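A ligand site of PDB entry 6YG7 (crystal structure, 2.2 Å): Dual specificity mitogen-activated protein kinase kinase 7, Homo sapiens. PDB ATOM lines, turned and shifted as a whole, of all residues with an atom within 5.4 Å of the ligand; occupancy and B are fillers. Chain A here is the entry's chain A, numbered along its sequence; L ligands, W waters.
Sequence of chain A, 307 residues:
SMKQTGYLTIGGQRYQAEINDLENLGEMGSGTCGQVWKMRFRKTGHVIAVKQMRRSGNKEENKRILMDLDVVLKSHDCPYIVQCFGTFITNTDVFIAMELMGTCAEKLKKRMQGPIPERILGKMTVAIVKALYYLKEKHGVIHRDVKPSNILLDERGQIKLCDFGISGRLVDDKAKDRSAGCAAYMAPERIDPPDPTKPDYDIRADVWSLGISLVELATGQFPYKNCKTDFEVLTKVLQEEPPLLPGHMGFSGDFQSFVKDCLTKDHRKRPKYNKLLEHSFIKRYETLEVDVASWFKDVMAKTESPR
The side-chain sulfur (SG) of Cys 104 is bonded to a carbon (C15) of the ligand, at 1.6 Å.
N of Asp 163 is in hydrogen-bond range of O3 of the ligand.
O of Asp 163 sits at hydrogen-bond distance from N5 of the ligand, at 3.1 Å.
O of Ile 142 sits close to N7 of the ligand.
A nitrogen (N7) of the ligand lies close to the backbone carbonyl oxygen (O) of His 143, 3.1 Å away.
N of Met 101 lies within hydrogen-bond range of N1 of the ligand, 3.1 Å away.
The backbone carbonyl oxygen (O) of Met 101 lies within hydrogen-bond range of a nitrogen (N3) of the ligand, at 3.3 Å.
O of Cys 162 is in hydrogen-bond range of NE2 of His 143 (2.7 Å).
N of Val 82 sits at hydrogen-bond distance from O of Leu 161, at 3.1 Å.
The backbone NH (N) of Met 98 sits at hydrogen-bond distance from the backbone carbonyl oxygen (O) of Ala 49.
N of Ile 96 sits at hydrogen-bond distance from O of Lys 51, 2.7 Å away.
The backbone NH of Met 28 lies within hydrogen-bond range of the backbone carbonyl oxygen of Val 36, at 2.9 Å.
The backbone NH (N) of Val 141 lies within hydrogen-bond range of the backbone carbonyl oxygen (O) of Leu 135, 3.0 Å away.
A fluorine (F1) of the ligand sits close to the backbone carbonyl oxygen (O) of Leu 161.
CG1 of Val 36 touches C22 of the ligand (3.9 Å).
Lys 51 touches the ligand.
Asp 68 touches the ligand (OD2 to C30, 3.5 Å).
Ile 81 touches the ligand (CG2 to F1, 3.8 Å).
CG1 of Val 82 touches O3 of the ligand, at 3.4 Å.
Met 98 touches the ligand.
O of Glu 99 touches C21 of the ligand, 3.1 Å away.
Leu 100 touches the ligand.
CE of Lys 107 touches O1 of the ligand, 3.2 Å away.
Leu 135 touches the ligand.
Arg 144 touches the ligand (NH1 to C31, 3.8 Å).
Ser 149 touches the ligand (O to C15, 3.8 Å).
Leu 152 touches the ligand.
Cys 162 touches the ligand.
CZ of Phe 164 touches N2 of the ligand (3.1 Å).
Hydrophobic or aromatic side chains that line the ligand: Val 36, Ile 81, Val 82, Met 98, Met 101, Leu 135, His 143, Leu 152 and Phe 164.
Within 4 Å of the ligand: Val 36, Lys 51, Asp 68, Ile 81, Val 82, Met 98, Glu 99, Leu 100, Met 101, Cys 104, Lys 107, Leu 135, Ile 142, His 143, Arg 144, Ser 149, Leu 152, Leu 161, Cys 162, Asp 163 and Phe 164.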
ATOM      1  N   MET A  28     -33.171   9.864   5.221  1.00  0.00           N
ATOM      2  CA  MET A  28     -32.029  10.165   6.113  1.00  0.00           C
ATOM      3  C   MET A  28     -32.125  11.544   6.796  1.00  0.00           C
ATOM      4  O   MET A  28     -31.702  11.663   7.936  1.00  0.00           O
ATOM      5  CB  MET A  28     -30.731  10.095   5.329  1.00  0.00           C
ATOM      6  CG  MET A  28     -30.328   8.700   4.928  1.00  0.00           C
ATOM      7  SD  MET A  28     -28.710   8.718   4.090  1.00  0.00           S
ATOM      8  CE  MET A  28     -29.157   9.526   2.577  1.00  0.00           C
ATOM      9  N   GLY A  29     -32.627  12.564   6.094  1.00  0.00           N
ATOM     10  CA  GLY A  29     -32.710  13.927   6.659  1.00  0.00           C
ATOM     11  C   GLY A  29     -33.895  14.177   7.575  1.00  0.00           C
ATOM     12  O   GLY A  29     -34.625  13.245   7.940  1.00  0.00           O
ATOM     13  N   VAL A  36     -34.125  13.967   1.551  1.00  0.00           N
ATOM     14  CA  VAL A  36     -32.991  13.062   1.280  1.00  0.00           C
ATOM     15  C   VAL A  36     -33.289  11.603   1.639  1.00  0.00           C
ATOM     16  O   VAL A  36     -33.695  11.323   2.756  1.00  0.00           O
ATOM     17  CB  VAL A  36     -31.703  13.497   2.028  1.00  0.00           C
ATOM     18  CG1 VAL A  36     -30.535  12.600   1.641  1.00  0.00           C
ATOM     19  CG2 VAL A  36     -31.340  14.941   1.678  1.00  0.00           C
ATOM     20  N   ALA A  49     -26.992   8.209  -1.778  1.00  0.00           N
ATOM     21  CA  ALA A  49     -27.836   9.259  -1.179  1.00  0.00           C
ATOM     22  C   ALA A  49     -28.485  10.044  -2.285  1.00  0.00           C
ATOM     23  O   ALA A  49     -27.813  10.457  -3.249  1.00  0.00           O
ATOM     24  CB  ALA A  49     -27.038  10.157  -0.243  1.00  0.00           C
ATOM     25  N   VAL A  50     -29.799  10.245  -2.179  1.00  0.00           N
ATOM     26  CA  VAL A  50     -30.540  10.979  -3.194  1.00  0.00           C
ATOM     27  C   VAL A  50     -31.293  12.158  -2.599  1.00  0.00           C
ATOM     28  O   VAL A  50     -32.121  12.000  -1.706  1.00  0.00           O
ATOM     29  CB  VAL A  50     -31.541  10.088  -3.883  1.00  0.00           C
ATOM     30  CG1 VAL A  50     -32.224  10.858  -4.994  1.00  0.00           C
ATOM     31  CG2 VAL A  50     -30.836   8.868  -4.492  1.00  0.00           C
ATOM     32  N   LYS A  51     -31.037  13.345  -3.143  1.00  0.00           N
ATOM     33  CA  LYS A  51     -31.804  14.515  -2.815  1.00  0.00           C
ATOM     34  C   LYS A  51     -32.925  14.760  -3.839  1.00  0.00           C
ATOM     35  O   LYS A  51     -32.700  14.803  -5.051  1.00  0.00           O
ATOM     36  CB  LYS A  51     -30.932  15.737  -2.752  1.00  0.00           C
ATOM     37  CG  LYS A  51     -31.649  16.999  -2.251  1.00  0.00           C
ATOM     38  CD  LYS A  51     -30.610  18.016  -1.785  1.00  0.00           C
ATOM     39  CE  LYS A  51     -31.106  19.456  -1.860  1.00  0.00           C
ATOM     40  NZ  LYS A  51     -32.077  19.741  -0.801  1.00  0.00           N
ATOM     41  N   ASP A  68     -24.821  25.034  -9.322  1.00  0.00           N
ATOM     42  CA  ASP A  68     -24.111  24.366  -8.237  1.00  0.00           C
ATOM     43  C   ASP A  68     -23.871  22.887  -8.543  1.00  0.00           C
ATOM     44  O   ASP A  68     -22.791  22.384  -8.285  1.00  0.00           O
ATOM     45  CB  ASP A  68     -24.862  24.513  -6.926  1.00  0.00           C
ATOM     46  CG  ASP A  68     -24.619  25.874  -6.257  1.00  0.00           C
ATOM     47  OD1 ASP A  68     -24.026  26.791  -6.882  1.00  0.00           O
ATOM     48  OD2 ASP A  68     -25.065  26.038  -5.114  1.00  0.00           O
ATOM     49  N   LEU A  69     -24.865  22.198  -9.098  1.00  0.00           N
ATOM     50  CA  LEU A  69     -24.667  20.828  -9.585  1.00  0.00           C
ATOM     51  C   LEU A  69     -23.555  20.745 -10.628  1.00  0.00           C
ATOM     52  O   LEU A  69     -22.797  19.783 -10.670  1.00  0.00           O
ATOM     53  CB  LEU A  69     -25.953  20.256 -10.214  1.00  0.00           C
ATOM     54  CG  LEU A  69     -27.137  20.018  -9.269  1.00  0.00           C
ATOM     55  CD1 LEU A  69     -28.237  19.261 -10.016  1.00  0.00           C
ATOM     56  CD2 LEU A  69     -26.692  19.262  -8.016  1.00  0.00           C
ATOM     57  N   VAL A  71     -20.939  22.429 -10.835  1.00  0.00           N
ATOM     58  CA  VAL A  71     -19.659  22.457 -10.143  1.00  0.00           C
ATOM     59  C   VAL A  71     -19.315  21.107  -9.514  1.00  0.00           C
ATOM     60  O   VAL A  71     -18.200  20.621  -9.683  1.00  0.00           O
ATOM     61  CB  VAL A  71     -19.622  23.571  -9.076  1.00  0.00           C
ATOM     62  CG1 VAL A  71     -18.348  23.465  -8.259  1.00  0.00           C
ATOM     63  CG2 VAL A  71     -19.723  24.949  -9.733  1.00  0.00           C
ATOM     64  N   VAL A  72     -20.260  20.522  -8.789  1.00  0.00           N
ATOM     65  CA  VAL A  72     -19.995  19.261  -8.116  1.00  0.00           C
ATOM     66  C   VAL A  72     -19.783  18.138  -9.147  1.00  0.00           C
ATOM     67  O   VAL A  72     -18.798  17.414  -9.066  1.00  0.00           O
ATOM     68  CB  VAL A  72     -21.031  18.919  -7.002  1.00  0.00           C
ATOM     69  CG1 VAL A  72     -22.440  18.758  -7.546  1.00  0.00           C
ATOM     70  CG2 VAL A  72     -20.630  17.662  -6.281  1.00  0.00           C
ATOM     71  N   ILE A  81     -14.107  16.453  -2.183  1.00  0.00           N
ATOM     72  CA  ILE A  81     -15.443  16.930  -2.432  1.00  0.00           C
ATOM     73  C   ILE A  81     -16.365  15.748  -2.675  1.00  0.00           C
ATOM     74  O   ILE A  81     -16.082  14.897  -3.497  1.00  0.00           O
ATOM     75  CB  ILE A  81     -15.453  17.873  -3.621  1.00  0.00           C
ATOM     76  CG1 ILE A  81     -14.880  19.233  -3.183  1.00  0.00           C
ATOM     77  CG2 ILE A  81     -16.876  18.048  -4.179  1.00  0.00           C
ATOM     78  CD1 ILE A  81     -14.434  20.113  -4.306  1.00  0.00           C
ATOM     79  N   VAL A  82     -17.508  15.779  -1.994  1.00  0.00           N
ATOM     80  CA  VAL A  82     -18.528  14.767  -2.185  1.00  0.00           C
ATOM     81  C   VAL A  82     -18.946  14.593  -3.706  1.00  0.00           C
ATOM     82  O   VAL A  82     -19.204  15.541  -4.422  1.00  0.00           O
ATOM     83  CB  VAL A  82     -19.761  15.040  -1.257  1.00  0.00           C
ATOM     84  CG1 VAL A  82     -20.600  16.224  -1.740  1.00  0.00           C
ATOM     85  CG2 VAL A  82     -20.615  13.795  -1.176  1.00  0.00           C
ATOM     86  N   ILE A  96     -31.142  14.195  -7.231  1.00  0.00           N
ATOM     87  CA  ILE A  96     -29.689  14.333  -7.299  1.00  0.00           C
ATOM     88  C   ILE A  96     -29.059  13.177  -6.515  1.00  0.00           C
ATOM     89  O   ILE A  96     -29.334  13.013  -5.354  1.00  0.00           O
ATOM     90  CB  ILE A  96     -29.226  15.657  -6.713  1.00  0.00           C
ATOM     91  CG1 ILE A  96     -29.968  16.829  -7.393  1.00  0.00           C
ATOM     92  CG2 ILE A  96     -27.701  15.793  -6.856  1.00  0.00           C
ATOM     93  CD1 ILE A  96     -30.047  18.022  -6.474  1.00  0.00           C
ATOM     94  N   MET A  98     -25.950  11.169  -4.995  1.00  0.00           N
ATOM     95  CA  MET A  98     -24.665  11.382  -4.435  1.00  0.00           C
ATOM     96  C   MET A  98     -24.134  10.115  -3.759  1.00  0.00           C
ATOM     97  O   MET A  98     -24.912   9.185  -3.356  1.00  0.00           O
ATOM     98  CB  MET A  98     -24.723  12.486  -3.390  1.00  0.00           C
ATOM     99  CG  MET A  98     -25.397  13.750  -3.855  1.00  0.00           C
ATOM    100  SD  MET A  98     -24.442  14.736  -5.041  1.00  0.00           S
ATOM    101  CE  MET A  98     -23.096  15.289  -3.994  1.00  0.00           C
ATOM    102  N   GLU A  99     -22.795  10.038  -3.672  1.00  0.00           N
ATOM    103  CA  GLU A  99     -22.140   9.000  -2.853  1.00  0.00           C
ATOM    104  C   GLU A  99     -22.614   9.162  -1.442  1.00  0.00           C
ATOM    105  O   GLU A  99     -22.758  10.254  -1.001  1.00  0.00           O
ATOM    106  CB  GLU A  99     -20.614   9.085  -2.953  1.00  0.00           C
ATOM    107  CG  GLU A  99     -19.985  10.204  -2.180  1.00  0.00           C
ATOM    108  CD  GLU A  99     -18.449  10.178  -2.251  1.00  0.00           C
ATOM    109  OE1 GLU A  99     -17.851   9.133  -1.995  1.00  0.00           O
ATOM    110  OE2 GLU A  99     -17.841  11.223  -2.535  1.00  0.00           O
ATOM    111  N   LEU A 100     -22.923   8.067  -0.763  1.00  0.00           N
ATOM    112  CA  LEU A 100     -23.454   8.116   0.582  1.00  0.00           C
ATOM    113  C   LEU A 100     -22.284   8.193   1.526  1.00  0.00           C
ATOM    114  O   LEU A 100     -21.378   7.374   1.486  1.00  0.00           O
ATOM    115  CB  LEU A 100     -24.299   6.887   0.885  1.00  0.00           C
ATOM    116  CG  LEU A 100     -24.923   6.759   2.270  1.00  0.00           C
ATOM    117  CD1 LEU A 100     -25.737   7.965   2.605  1.00  0.00           C
ATOM    118  CD2 LEU A 100     -25.831   5.559   2.379  1.00  0.00           C
ATOM    119  N   MET A 101     -22.272   9.183   2.363  1.00  0.00           N
ATOM    120  CA  MET A 101     -21.236   9.267   3.403  1.00  0.00           C
ATOM    121  C   MET A 101     -21.940   8.892   4.662  1.00  0.00           C
ATOM    122  O   MET A 101     -23.137   9.183   4.803  1.00  0.00           O
ATOM    123  CB  MET A 101     -20.729  10.695   3.534  1.00  0.00           C
ATOM    124  CG  MET A 101     -20.084  11.234   2.278  1.00  0.00           C
ATOM    125  SD  MET A 101     -18.603  10.350   1.896  1.00  0.00           S
ATOM    126  CE  MET A 101     -17.380  11.309   2.796  1.00  0.00           C
ATOM    127  N   GLY A 102     -21.206   8.279   5.577  1.00  0.00           N
ATOM    128  CA  GLY A 102     -21.805   7.763   6.798  1.00  0.00           C
ATOM    129  C   GLY A 102     -22.480   8.831   7.593  1.00  0.00           C
ATOM    130  O   GLY A 102     -23.637   8.682   7.978  1.00  0.00           O
ATOM    131  N   THR A 103     -21.764   9.925   7.872  1.00  0.00           N
ATOM    132  CA  THR A 103     -22.345  10.991   8.657  1.00  0.00           C
ATOM    133  C   THR A 103     -21.519  12.314   8.498  1.00  0.00           C
ATOM    134  O   THR A 103     -20.625  12.405   7.659  1.00  0.00           O
ATOM    135  CB  THR A 103     -22.488  10.565  10.126  1.00  0.00           C
ATOM    136  OG1 THR A 103     -23.287  11.503  10.840  1.00  0.00           O
ATOM    137  CG2 THR A 103     -21.131  10.471  10.768  1.00  0.00           C
ATOM    138  N   CYS A 104     -21.895  13.335   9.254  1.00  0.00           N
ATOM    139  CA  CYS A 104     -21.183  14.590   9.201  1.00  0.00           C
ATOM    140  C   CYS A 104     -20.544  14.889  10.548  1.00  0.00           C
ATOM    141  O   CYS A 104     -20.885  14.263  11.558  1.00  0.00           O
ATOM    142  CB  CYS A 104     -22.119  15.702   8.811  1.00  0.00           C
ATOM    143  SG  CYS A 104     -23.533  15.850   9.880  1.00  0.00           S
ATOM    144  N   GLU A 106     -20.886  17.417  12.526  1.00  0.00           N
ATOM    145  CA  GLU A 106     -21.861  17.841  13.533  1.00  0.00           C
ATOM    146  C   GLU A 106     -22.394  16.672  14.343  1.00  0.00           C
ATOM    147  O   GLU A 106     -22.531  16.770  15.559  1.00  0.00           O
ATOM    148  CB  GLU A 106     -23.021  18.570  12.878  1.00  0.00           C
ATOM    149  CG  GLU A 106     -24.072  19.101  13.836  1.00  0.00           C
ATOM    150  CD  GLU A 106     -25.389  19.430  13.141  1.00  0.00           C
ATOM    151  OE1 GLU A 106     -25.870  20.575  13.348  1.00  0.00           O
ATOM    152  OE2 GLU A 106     -25.952  18.561  12.400  1.00  0.00           O
ATOM    153  N   LYS A 107     -22.685  15.556  13.671  1.00  0.00           N
ATOM    154  CA  LYS A 107     -23.319  14.448  14.326  1.00  0.00           C
ATOM    155  C   LYS A 107     -22.290  13.645  15.064  1.00  0.00           C
ATOM    156  O   LYS A 107     -22.603  13.068  16.092  1.00  0.00           O
ATOM    157  CB  LYS A 107     -24.076  13.563  13.353  1.00  0.00           C
ATOM    158  CG  LYS A 107     -25.380  14.150  12.900  1.00  0.00           C
ATOM    159  CD  LYS A 107     -26.091  13.202  11.967  1.00  0.00           C
ATOM    160  CE  LYS A 107     -27.147  13.883  11.103  1.00  0.00           C
ATOM    161  NZ  LYS A 107     -28.513  13.672  11.632  1.00  0.00           N
ATOM    162  N   LEU A 135     -12.089  24.330  -5.226  1.00  0.00           N
ATOM    163  CA  LEU A 135     -13.267  25.038  -5.718  1.00  0.00           C
ATOM    164  C   LEU A 135     -12.966  26.410  -6.248  1.00  0.00           C
ATOM    165  O   LEU A 135     -13.534  26.841  -7.256  1.00  0.00           O
ATOM    166  CB  LEU A 135     -14.323  25.157  -4.630  1.00  0.00           C
ATOM    167  CG  LEU A 135     -15.094  23.867  -4.338  1.00  0.00           C
ATOM    168  CD1 LEU A 135     -16.013  24.101  -3.144  1.00  0.00           C
ATOM    169  CD2 LEU A 135     -15.906  23.390  -5.542  1.00  0.00           C
ATOM    170  N   VAL A 141     -15.320  29.268  -7.646  1.00  0.00           N
ATOM    171  CA  VAL A 141     -16.440  29.375  -6.698  1.00  0.00           C
ATOM    172  C   VAL A 141     -15.961  29.346  -5.282  1.00  0.00           C
ATOM    173  O   VAL A 141     -14.943  28.736  -4.956  1.00  0.00           O
ATOM    174  CB  VAL A 141     -17.570  28.320  -6.899  1.00  0.00           C
ATOM    175  CG1 VAL A 141     -18.114  28.435  -8.320  1.00  0.00           C
ATOM    176  CG2 VAL A 141     -17.140  26.882  -6.611  1.00  0.00           C
ATOM    177  N   ILE A 142     -16.766  29.973  -4.452  1.00  0.00           N
ATOM    178  CA  ILE A 142     -16.567  30.033  -3.044  1.00  0.00           C
ATOM    179  C   ILE A 142     -17.693  29.167  -2.427  1.00  0.00           C
ATOM    180  O   ILE A 142     -18.700  28.925  -3.082  1.00  0.00           O
ATOM    181  CB  ILE A 142     -16.595  31.527  -2.605  1.00  0.00           C
ATOM    182  CG1 ILE A 142     -16.011  31.717  -1.233  1.00  0.00           C
ATOM    183  CG2 ILE A 142     -17.995  32.073  -2.601  1.00  0.00           C
ATOM    184  CD1 ILE A 142     -16.248  33.078  -0.618  1.00  0.00           C
ATOM    185  N   HIS A 143     -17.514  28.667  -1.203  1.00  0.00           N
ATOM    186  CA  HIS A 143     -18.537  27.810  -0.607  1.00  0.00           C
ATOM    187  C   HIS A 143     -19.672  28.586   0.047  1.00  0.00           C
ATOM    188  O   HIS A 143     -20.801  28.400  -0.321  1.00  0.00           O
ATOM    189  CB  HIS A 143     -17.903  26.845   0.383  1.00  0.00           C
ATOM    190  CG  HIS A 143     -18.803  25.732   0.824  1.00  0.00           C
ATOM    191  ND1 HIS A 143     -19.698  25.874   1.859  1.00  0.00           N
ATOM    192  CD2 HIS A 143     -18.923  24.476   0.388  1.00  0.00           C
ATOM    193  CE1 HIS A 143     -20.351  24.737   2.033  1.00  0.00           C
ATOM    194  NE2 HIS A 143     -19.881  23.870   1.159  1.00  0.00           N
ATOM    195  N   ARG A 144     -19.341  29.385   1.065  1.00  0.00           N
ATOM    196  CA  ARG A 144     -20.246  30.346   1.781  1.00  0.00           C
ATOM    197  C   ARG A 144     -21.012  29.750   2.947  1.00  0.00           C
ATOM    198  O   ARG A 144     -21.709  30.450   3.628  1.00  0.00           O
ATOM    199  CB  ARG A 144     -21.251  31.071   0.842  1.00  0.00           C
ATOM    200  CG  ARG A 144     -20.660  31.922  -0.258  1.00  0.00           C
ATOM    201  CD  ARG A 144     -21.742  32.691  -1.055  1.00  0.00           C
ATOM    202  NE  ARG A 144     -21.246  33.145  -2.378  1.00  0.00           N
ATOM    203  CZ  ARG A 144     -21.991  33.510  -3.427  1.00  0.00           C
ATOM    204  NH1 ARG A 144     -23.326  33.495  -3.393  1.00  0.00           N
ATOM    205  NH2 ARG A 144     -21.378  33.889  -4.548  1.00  0.00           N
ATOM    206  N   SER A 149     -21.727  20.621   9.880  1.00  0.00           N
ATOM    207  CA  SER A 149     -22.732  19.797   9.248  1.00  0.00           C
ATOM    208  C   SER A 149     -22.450  19.609   7.738  1.00  0.00           C
ATOM    209  O   SER A 149     -23.017  18.709   7.095  1.00  0.00           O
ATOM    210  CB  SER A 149     -24.162  20.287   9.540  1.00  0.00           C
ATOM    211  OG  SER A 149     -24.379  21.565   8.982  1.00  0.00           O
ATOM    212  N   LEU A 152     -18.312  15.873   5.780  1.00  0.00           N
ATOM    213  CA  LEU A 152     -18.757  14.475   5.777  1.00  0.00           C
ATOM    214  C   LEU A 152     -17.617  13.517   6.007  1.00  0.00           C
ATOM    215  O   LEU A 152     -16.516  13.728   5.496  1.00  0.00           O
ATOM    216  CB  LEU A 152     -19.399  14.136   4.445  1.00  0.00           C
ATOM    217  CG  LEU A 152     -20.589  14.986   4.085  1.00  0.00           C
ATOM    218  CD1 LEU A 152     -21.184  14.548   2.758  1.00  0.00           C
ATOM    219  CD2 LEU A 152     -21.645  14.922   5.151  1.00  0.00           C
ATOM    220  N   LEU A 161     -15.895  17.707   1.803  1.00  0.00           N
ATOM    221  CA  LEU A 161     -16.753  18.876   1.857  1.00  0.00           C
ATOM    222  C   LEU A 161     -18.028  18.631   1.092  1.00  0.00           C
ATOM    223  O   LEU A 161     -18.021  18.148  -0.041  1.00  0.00           O
ATOM    224  CB  LEU A 161     -16.008  20.059   1.218  1.00  0.00           C
ATOM    225  CG  LEU A 161     -16.703  21.410   1.277  1.00  0.00           C
ATOM    226  CD1 LEU A 161     -16.905  21.897   2.690  1.00  0.00           C
ATOM    227  CD2 LEU A 161     -15.900  22.403   0.466  1.00  0.00           C
ATOM    228  N   CYS A 162     -19.139  19.047   1.677  1.00  0.00           N
ATOM    229  CA  CYS A 162     -20.395  19.024   0.963  1.00  0.00           C
ATOM    230  C   CYS A 162     -21.137  20.341   1.204  1.00  0.00           C
ATOM    231  O   CYS A 162     -20.564  21.296   1.776  1.00  0.00           O
ATOM    232  CB  CYS A 162     -21.163  17.799   1.409  1.00  0.00           C
ATOM    233  SG  CYS A 162     -21.993  18.029   2.965  1.00  0.00           S
ATOM    234  N   ASP A 163     -22.370  20.417   0.693  1.00  0.00           N
ATOM    235  CA  ASP A 163     -23.276  21.551   0.967  1.00  0.00           C
ATOM    236  C   ASP A 163     -24.686  21.071   1.019  1.00  0.00           C
ATOM    237  O   ASP A 163     -25.296  20.869  -0.026  1.00  0.00           O
ATOM    238  CB  ASP A 163     -23.146  22.641  -0.073  1.00  0.00           C
ATOM    239  CG  ASP A 163     -23.919  23.902   0.277  1.00  0.00           C
ATOM    240  OD1 ASP A 163     -24.595  23.946   1.346  1.00  0.00           O
ATOM    241  OD2 ASP A 163     -23.858  24.870  -0.498  1.00  0.00           O
ATOM    242  N   PHE A 164     -25.187  20.872   2.234  1.00  0.00           N
ATOM    243  CA  PHE A 164     -26.561  20.439   2.477  1.00  0.00           C
ATOM    244  C   PHE A 164     -27.600  21.492   2.256  1.00  0.00           C
ATOM    245  O   PHE A 164     -28.755  21.159   2.297  1.00  0.00           O
ATOM    246  CB  PHE A 164     -26.750  19.948   3.929  1.00  0.00           C
ATOM    247  CG  PHE A 164     -26.477  18.519   4.097  1.00  0.00           C
ATOM    248  CD1 PHE A 164     -27.426  17.577   3.722  1.00  0.00           C
ATOM    249  CD2 PHE A 164     -25.275  18.092   4.637  1.00  0.00           C
ATOM    250  CE1 PHE A 164     -27.190  16.220   3.877  1.00  0.00           C
ATOM    251  CE2 PHE A 164     -25.010  16.736   4.778  1.00  0.00           C
ATOM    252  CZ  PHE A 164     -25.988  15.807   4.412  1.00  0.00           C
HETATM  253  C1  LIG L   1     -23.889  21.372  -3.656  1.00  0.00           C
HETATM  254  C2  LIG L   1     -23.349  20.298  -2.967  1.00  0.00           C
HETATM  255  C3  LIG L   1     -21.980  20.311  -2.662  1.00  0.00           C
HETATM  256  N1  LIG L   1     -24.048  11.723   2.152  1.00  0.00           N
HETATM  257  C4  LIG L   1     -24.081  18.318  -1.651  1.00  0.00           C
HETATM  258  C5  LIG L   1     -25.143  17.277  -1.546  1.00  0.00           C
HETATM  259  N2  LIG L   1     -25.788  13.297   2.619  1.00  0.00           N
HETATM  260  C6  LIG L   1     -26.130  17.042  -2.500  1.00  0.00           C
HETATM  261  C7  LIG L   1     -27.094  16.072  -2.271  1.00  0.00           C
HETATM  262  C8  LIG L   1     -27.117  15.324  -1.111  1.00  0.00           C
HETATM  263  C9  LIG L   1     -26.135  15.594  -0.145  1.00  0.00           C
HETATM  264  N3  LIG L   1     -25.140  11.698   4.155  1.00  0.00           N
HETATM  265  C10 LIG L   1     -25.145  16.525  -0.373  1.00  0.00           C
HETATM  266  C11 LIG L   1     -25.518  13.884   1.453  1.00  0.00           C
HETATM  267  C12 LIG L   1     -24.515  13.475   0.569  1.00  0.00           C
HETATM  268  N4  LIG L   1     -26.529  13.729   6.799  1.00  0.00           N
HETATM  269  O1  LIG L   1     -27.398  15.265   8.198  1.00  0.00           O
HETATM  270  C13 LIG L   1     -26.413  14.713   7.732  1.00  0.00           C
HETATM  271  C14 LIG L   1     -25.026  15.063   8.212  1.00  0.00           C
HETATM  272  C15 LIG L   1     -24.956  16.251   9.218  1.00  0.00           C
HETATM  273  C16 LIG L   1     -25.400  12.945   6.284  1.00  0.00           C
HETATM  274  C17 LIG L   1     -27.815  13.341   6.193  1.00  0.00           C
HETATM  275  C18 LIG L   1     -27.390  12.581   4.935  1.00  0.00           C
HETATM  276  C19 LIG L   1     -26.020  11.964   5.298  1.00  0.00           C
HETATM  277  C20 LIG L   1     -25.017  12.247   2.924  1.00  0.00           C
HETATM  278  C21 LIG L   1     -23.810  12.371   1.002  1.00  0.00           C
HETATM  279  O2  LIG L   1     -26.250  14.986   1.108  1.00  0.00           O
HETATM  280  C22 LIG L   1     -28.115  14.226  -0.907  1.00  0.00           C
HETATM  281  O3  LIG L   1     -23.107  18.289  -0.918  1.00  0.00           O
HETATM  282  N5  LIG L   1     -24.293  19.331  -2.530  1.00  0.00           N
HETATM  283  C23 LIG L   1     -21.160  21.366  -3.046  1.00  0.00           C
HETATM  284  C24 LIG L   1     -19.691  21.256  -2.650  1.00  0.00           C
HETATM  285  F1  LIG L   1     -19.366  20.072  -2.126  1.00  0.00           F
HETATM  286  F2  LIG L   1     -19.353  22.123  -1.708  1.00  0.00           F
HETATM  287  F3  LIG L   1     -18.829  21.415  -3.675  1.00  0.00           F
HETATM  288  C25 LIG L   1     -23.082  22.421  -4.038  1.00  0.00           C
HETATM  289  C26 LIG L   1     -21.713  22.435  -3.770  1.00  0.00           C
HETATM  290  C27 LIG L   1     -20.927  23.518  -4.466  1.00  0.00           C
HETATM  291  N6  LIG L   1     -20.921  24.849  -3.850  1.00  0.00           N
HETATM  292  C28 LIG L   1     -22.081  25.119  -2.999  1.00  0.00           C
HETATM  293  C29 LIG L   1     -21.903  26.416  -2.248  1.00  0.00           C
HETATM  294  N7  LIG L   1     -21.579  27.545  -3.156  1.00  0.00           N
HETATM  295  C30 LIG L   1     -22.746  28.239  -3.662  1.00  0.00           C
HETATM  296  C31 LIG L   1     -22.651  29.725  -3.405  1.00  0.00           C
HETATM  297  C32 LIG L   1     -20.587  27.212  -4.218  1.00  0.00           C
HETATM  298  C33 LIG L   1     -20.883  25.897  -4.857  1.00  0.00           C
HETATM  299  O   HOH W   1     -27.022  20.006  -4.169  1.00  0.00           O
